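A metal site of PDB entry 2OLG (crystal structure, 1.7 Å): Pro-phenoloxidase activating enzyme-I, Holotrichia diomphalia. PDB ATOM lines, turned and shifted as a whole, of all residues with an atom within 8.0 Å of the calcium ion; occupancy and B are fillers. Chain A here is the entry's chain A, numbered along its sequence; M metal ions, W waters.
Four residues have an atom within 4 Å of the calcium ion: Glu 88, Asn 90, Thr 93 and Asp 96. The nearest printed residue that does not touch the calcium ion is Thr 91 (4.3 Å).
The calcium ion is bound by the backbone carbonyl oxygen (O) of Asn 90 (2.3 Å), water W2 (2.3 Å), water W1 (2.4 Å), the side-chain carboxylate (OE2) of Glu 88 (2.4 Å), the backbone carbonyl oxygen (O) of Thr 93 (2.4 Å), the side-chain carboxylate (OD1) of Asp 96 (2.5 Å) and the side-chain carboxylate (OD2) of Asp 96 (2.7 Å). The calcium ion has seven donor atoms within binding distance.
The side-chain amide nitrogen (ND2) of Asn 90 lies within hydrogen-bond range of the side-chain hydroxyl (OG1) of Thr 93, at 3.4 Å. The side-chain carboxylate (OD2) of Asp 96 lies close to the backbone NH (N) of Trp 89, 3.5 Å away. N of Ala 92 sits at hydrogen-bond distance from OD1 of Asn 90, 3.1 Å away. OD1 of Asn 90 sits at hydrogen-bond distance from OG1 of Thr 182, at 2.9 Å. The backbone NH (N) of Val 105 is in hydrogen-bond range of the backbone carbonyl oxygen (O) of Asp 96 (2.7 Å). The guanidinium group of Arg 85 lies within salt-bridge range of the side-chain carboxylate of Glu 88 (2.8 Å).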
ATOM      1  N   ARG A  85      14.608 -17.009 -28.710  1.00  0.00           N
ATOM      2  CA  ARG A  85      15.893 -16.309 -28.733  1.00  0.00           C
ATOM      3  C   ARG A  85      17.046 -17.270 -28.613  1.00  0.00           C
ATOM      4  O   ARG A  85      17.065 -18.121 -27.718  1.00  0.00           O
ATOM      5  CB  ARG A  85      15.985 -15.291 -27.601  1.00  0.00           C
ATOM      6  CG  ARG A  85      17.368 -14.598 -27.538  1.00  0.00           C
ATOM      7  CD  ARG A  85      17.338 -13.448 -26.571  1.00  0.00           C
ATOM      8  NE  ARG A  85      16.583 -12.353 -27.147  1.00  0.00           N
ATOM      9  CZ  ARG A  85      16.495 -11.123 -26.611  1.00  0.00           C
ATOM     10  NH1 ARG A  85      17.147 -10.815 -25.497  1.00  0.00           N
ATOM     11  NH2 ARG A  85      15.763 -10.204 -27.223  1.00  0.00           N
ATOM     12  N   GLY A  87      21.457 -17.642 -28.727  1.00  0.00           N
ATOM     13  CA  GLY A  87      22.748 -16.950 -28.570  1.00  0.00           C
ATOM     14  C   GLY A  87      22.792 -15.963 -27.415  1.00  0.00           C
ATOM     15  O   GLY A  87      23.716 -15.147 -27.346  1.00  0.00           O
ATOM     16  N   GLU A  88      21.763 -15.983 -26.539  1.00  0.00           N
ATOM     17  CA  GLU A  88      21.731 -15.086 -25.386  1.00  0.00           C
ATOM     18  C   GLU A  88      22.631 -15.636 -24.271  1.00  0.00           C
ATOM     19  O   GLU A  88      22.868 -16.849 -24.146  1.00  0.00           O
ATOM     20  CB  GLU A  88      20.290 -14.926 -24.857  1.00  0.00           C
ATOM     21  CG  GLU A  88      20.090 -14.013 -23.635  1.00  0.00           C
ATOM     22  CD  GLU A  88      20.421 -12.570 -23.921  1.00  0.00           C
ATOM     23  OE1 GLU A  88      19.510 -11.845 -24.344  1.00  0.00           O
ATOM     24  OE2 GLU A  88      21.600 -12.185 -23.745  1.00  0.00           O
ATOM     25  N   TRP A  89      23.156 -14.734 -23.454  1.00  0.00           N
ATOM     26  CA  TRP A  89      23.882 -15.127 -22.268  1.00  0.00           C
ATOM     27  C   TRP A  89      23.351 -14.322 -21.072  1.00  0.00           C
ATOM     28  O   TRP A  89      22.765 -14.897 -20.166  1.00  0.00           O
ATOM     29  CB  TRP A  89      25.404 -14.999 -22.460  1.00  0.00           C
ATOM     30  CG  TRP A  89      26.149 -15.336 -21.228  1.00  0.00           C
ATOM     31  CD1 TRP A  89      26.135 -16.532 -20.549  1.00  0.00           C
ATOM     32  CD2 TRP A  89      26.952 -14.433 -20.452  1.00  0.00           C
ATOM     33  NE1 TRP A  89      26.925 -16.440 -19.417  1.00  0.00           N
ATOM     34  CE2 TRP A  89      27.444 -15.172 -19.335  1.00  0.00           C
ATOM     35  CE3 TRP A  89      27.323 -13.081 -20.601  1.00  0.00           C
ATOM     36  CZ2 TRP A  89      28.290 -14.599 -18.372  1.00  0.00           C
ATOM     37  CZ3 TRP A  89      28.159 -12.505 -19.628  1.00  0.00           C
ATOM     38  CH2 TRP A  89      28.631 -13.269 -18.525  1.00  0.00           C
ATOM     39  N   ASN A  90      23.565 -13.012 -21.079  1.00  0.00           N
ATOM     40  CA  ASN A  90      23.046 -12.109 -20.063  1.00  0.00           C
ATOM     41  C   ASN A  90      21.922 -11.243 -20.624  1.00  0.00           C
ATOM     42  O   ASN A  90      22.162 -10.382 -21.475  1.00  0.00           O
ATOM     43  CB  ASN A  90      24.200 -11.219 -19.541  1.00  0.00           C
ATOM     44  CG  ASN A  90      23.808 -10.447 -18.311  1.00  0.00           C
ATOM     45  OD1 ASN A  90      22.639 -10.476 -17.874  1.00  0.00           O
ATOM     46  ND2 ASN A  90      24.806  -9.784 -17.704  1.00  0.00           N
ATOM     47  N   THR A  91      20.685 -11.497 -20.221  1.00  0.00           N
ATOM     48  CA  THR A  91      19.531 -10.724 -20.744  1.00  0.00           C
ATOM     49  C   THR A  91      19.525  -9.268 -20.255  1.00  0.00           C
ATOM     50  O   THR A  91      18.781  -8.465 -20.769  1.00  0.00           O
ATOM     51  CB  THR A  91      18.221 -11.323 -20.308  1.00  0.00           C
ATOM     52  OG1 THR A  91      18.214 -11.347 -18.905  1.00  0.00           O
ATOM     53  CG2 THR A  91      18.060 -12.761 -20.823  1.00  0.00           C
ATOM     54  N   ALA A  92      20.343  -8.941 -19.255  1.00  0.00           N
ATOM     55  CA  ALA A  92      20.386  -7.575 -18.716  1.00  0.00           C
ATOM     56  C   ALA A  92      21.221  -6.661 -19.621  1.00  0.00           C
ATOM     57  O   ALA A  92      21.051  -5.436 -19.602  1.00  0.00           O
ATOM     58  CB  ALA A  92      20.946  -7.566 -17.306  1.00  0.00           C
ATOM     59  N   THR A  93      22.107  -7.258 -20.411  1.00  0.00           N
ATOM     60  CA  THR A  93      23.088  -6.459 -21.141  1.00  0.00           C
ATOM     61  C   THR A  93      23.085  -6.693 -22.632  1.00  0.00           C
ATOM     62  O   THR A  93      22.649  -7.746 -23.111  1.00  0.00           O
ATOM     63  CB  THR A  93      24.515  -6.679 -20.574  1.00  0.00           C
ATOM     64  OG1 THR A  93      24.905  -8.072 -20.653  1.00  0.00           O
ATOM     65  CG2 THR A  93      24.545  -6.291 -19.081  1.00  0.00           C
ATOM     66  N   ASP A  94      23.609  -5.729 -23.366  1.00  0.00           N
ATOM     67  CA  ASP A  94      23.958  -5.937 -24.771  1.00  0.00           C
ATOM     68  C   ASP A  94      24.873  -4.784 -25.172  1.00  0.00           C
ATOM     69  O   ASP A  94      24.500  -3.627 -25.042  1.00  0.00           O
ATOM     70  CB  ASP A  94      22.740  -5.991 -25.685  1.00  0.00           C
ATOM     71  CG  ASP A  94      23.095  -6.348 -27.121  1.00  0.00           C
ATOM     72  OD1 ASP A  94      23.578  -7.482 -27.396  1.00  0.00           O
ATOM     73  OD2 ASP A  94      22.918  -5.486 -27.998  1.00  0.00           O
ATOM     74  N   PRO A  95      26.100  -5.098 -25.596  1.00  0.00           N
ATOM     75  CA  PRO A  95      26.668  -6.427 -25.844  1.00  0.00           C
ATOM     76  C   PRO A  95      26.946  -7.198 -24.533  1.00  0.00           C
ATOM     77  O   PRO A  95      26.863  -6.634 -23.446  1.00  0.00           O
ATOM     78  CB  PRO A  95      28.002  -6.125 -26.564  1.00  0.00           C
ATOM     79  CG  PRO A  95      28.341  -4.766 -26.150  1.00  0.00           C
ATOM     80  CD  PRO A  95      27.082  -4.019 -25.826  1.00  0.00           C
ATOM     81  N   ASP A  96      27.238  -8.488 -24.656  1.00  0.00           N
ATOM     82  CA  ASP A  96      27.595  -9.286 -23.485  1.00  0.00           C
ATOM     83  C   ASP A  96      29.090  -9.392 -23.384  1.00  0.00           C
ATOM     84  O   ASP A  96      29.712  -9.964 -24.288  1.00  0.00           O
ATOM     85  CB  ASP A  96      26.989 -10.685 -23.567  1.00  0.00           C
ATOM     86  CG  ASP A  96      25.494 -10.679 -23.336  1.00  0.00           C
ATOM     87  OD1 ASP A  96      24.987  -9.647 -22.883  1.00  0.00           O
ATOM     88  OD2 ASP A  96      24.797 -11.687 -23.621  1.00  0.00           O
ATOM     89  N   CYS A  97      29.651  -8.830 -22.322  1.00  0.00           N
ATOM     90  CA  CYS A  97      31.093  -8.800 -22.087  1.00  0.00           C
ATOM     91  C   CYS A  97      31.451  -9.398 -20.723  1.00  0.00           C
ATOM     92  O   CYS A  97      30.724  -9.226 -19.730  1.00  0.00           O
ATOM     93  CB  CYS A  97      31.620  -7.359 -22.170  1.00  0.00           C
ATOM     94  SG  CYS A  97      31.042  -6.506 -23.621  1.00  0.00           S
ATOM     95  N   VAL A 105      30.907 -10.771 -26.580  1.00  0.00           N
ATOM     96  CA  VAL A 105      30.306 -11.620 -27.603  1.00  0.00           C
ATOM     97  C   VAL A 105      30.065 -10.775 -28.867  1.00  0.00           C
ATOM     98  O   VAL A 105      29.420  -9.729 -28.826  1.00  0.00           O
ATOM     99  CB  VAL A 105      29.002 -12.298 -27.105  1.00  0.00           C
ATOM    100  CG1 VAL A 105      28.346 -13.128 -28.184  1.00  0.00           C
ATOM    101  CG2 VAL A 105      29.315 -13.185 -25.910  1.00  0.00           C
ATOM    102  N   ASP A 107      28.366 -11.407 -31.489  1.00  0.00           N
ATOM    103  CA  ASP A 107      27.073 -11.644 -32.062  1.00  0.00           C
ATOM    104  C   ASP A 107      25.906 -11.263 -31.145  1.00  0.00           C
ATOM    105  O   ASP A 107      25.809 -11.737 -30.006  1.00  0.00           O
ATOM    106  CB  ASP A 107      26.976 -13.127 -32.439  1.00  0.00           C
ATOM    107  CG  ASP A 107      28.100 -13.579 -33.370  1.00  0.00           C
ATOM    108  OD1 ASP A 107      28.661 -12.711 -34.099  1.00  0.00           O
ATOM    109  OD2 ASP A 107      28.424 -14.785 -33.400  1.00  0.00           O
ATOM    110  N   LYS A 108      25.031 -10.406 -31.657  1.00  0.00           N
ATOM    111  CA  LYS A 108      23.812 -10.038 -30.964  1.00  0.00           C
ATOM    112  C   LYS A 108      22.894 -11.280 -30.922  1.00  0.00           C
ATOM    113  O   LYS A 108      22.883 -12.054 -31.884  1.00  0.00           O
ATOM    114  CB  LYS A 108      23.137  -8.913 -31.698  1.00  0.00           C
ATOM    115  CG  LYS A 108      22.005  -8.272 -30.955  1.00  0.00           C
ATOM    116  CD  LYS A 108      21.645  -6.912 -31.549  1.00  0.00           C
ATOM    117  CE  LYS A 108      20.511  -6.298 -30.756  1.00  0.00           C
ATOM    118  NZ  LYS A 108      19.634  -5.442 -31.613  1.00  0.00           N
ATOM    119  N   PRO A 109      22.165 -11.488 -29.818  1.00  0.00           N
ATOM    120  CA  PRO A 109      21.239 -12.644 -29.835  1.00  0.00           C
ATOM    121  C   PRO A 109      20.240 -12.560 -30.983  1.00  0.00           C
ATOM    122  O   PRO A 109      19.872 -11.468 -31.415  1.00  0.00           O
ATOM    123  CB  PRO A 109      20.531 -12.531 -28.481  1.00  0.00           C
ATOM    124  CG  PRO A 109      21.540 -11.850 -27.601  1.00  0.00           C
ATOM    125  CD  PRO A 109      22.172 -10.812 -28.509  1.00  0.00           C
ATOM    126  N   TRP A 172      17.594 -19.919 -17.121  1.00  0.00           N
ATOM    127  CA  TRP A 172      17.466 -18.566 -16.529  1.00  0.00           C
ATOM    128  C   TRP A 172      16.383 -18.461 -15.452  1.00  0.00           C
ATOM    129  O   TRP A 172      15.850 -17.380 -15.182  1.00  0.00           O
ATOM    130  CB  TRP A 172      17.198 -17.530 -17.605  1.00  0.00           C
ATOM    131  CG  TRP A 172      18.330 -17.218 -18.548  1.00  0.00           C
ATOM    132  CD1 TRP A 172      19.175 -16.149 -18.475  1.00  0.00           C
ATOM    133  CD2 TRP A 172      18.668 -17.924 -19.761  1.00  0.00           C
ATOM    134  NE1 TRP A 172      20.061 -16.153 -19.552  1.00  0.00           N
ATOM    135  CE2 TRP A 172      19.765 -17.221 -20.355  1.00  0.00           C
ATOM    136  CE3 TRP A 172      18.158 -19.083 -20.393  1.00  0.00           C
ATOM    137  CZ2 TRP A 172      20.338 -17.628 -21.547  1.00  0.00           C
ATOM    138  CZ3 TRP A 172      18.741 -19.499 -21.583  1.00  0.00           C
ATOM    139  CH2 TRP A 172      19.834 -18.779 -22.144  1.00  0.00           C
ATOM    140  N   THR A 182      19.215 -13.149 -14.857  1.00  0.00           N
ATOM    141  CA  THR A 182      19.596 -12.593 -16.163  1.00  0.00           C
ATOM    142  C   THR A 182      20.776 -13.306 -16.799  1.00  0.00           C
ATOM    143  O   THR A 182      20.905 -13.326 -18.022  1.00  0.00           O
ATOM    144  CB  THR A 182      19.818 -11.050 -16.150  1.00  0.00           C
ATOM    145  OG1 THR A 182      21.067 -10.739 -15.500  1.00  0.00           O
ATOM    146  CG2 THR A 182      18.624 -10.323 -15.459  1.00  0.00           C
HETATM  147 CA    CA M   1      22.688 -10.070 -23.721  1.00  0.00          CA
HETATM  148  O   HOH W   1      20.629  -9.562 -24.759  1.00  0.00           O
HETATM  149  O   HOH W   2      23.806  -9.572 -25.703  1.00  0.00           O
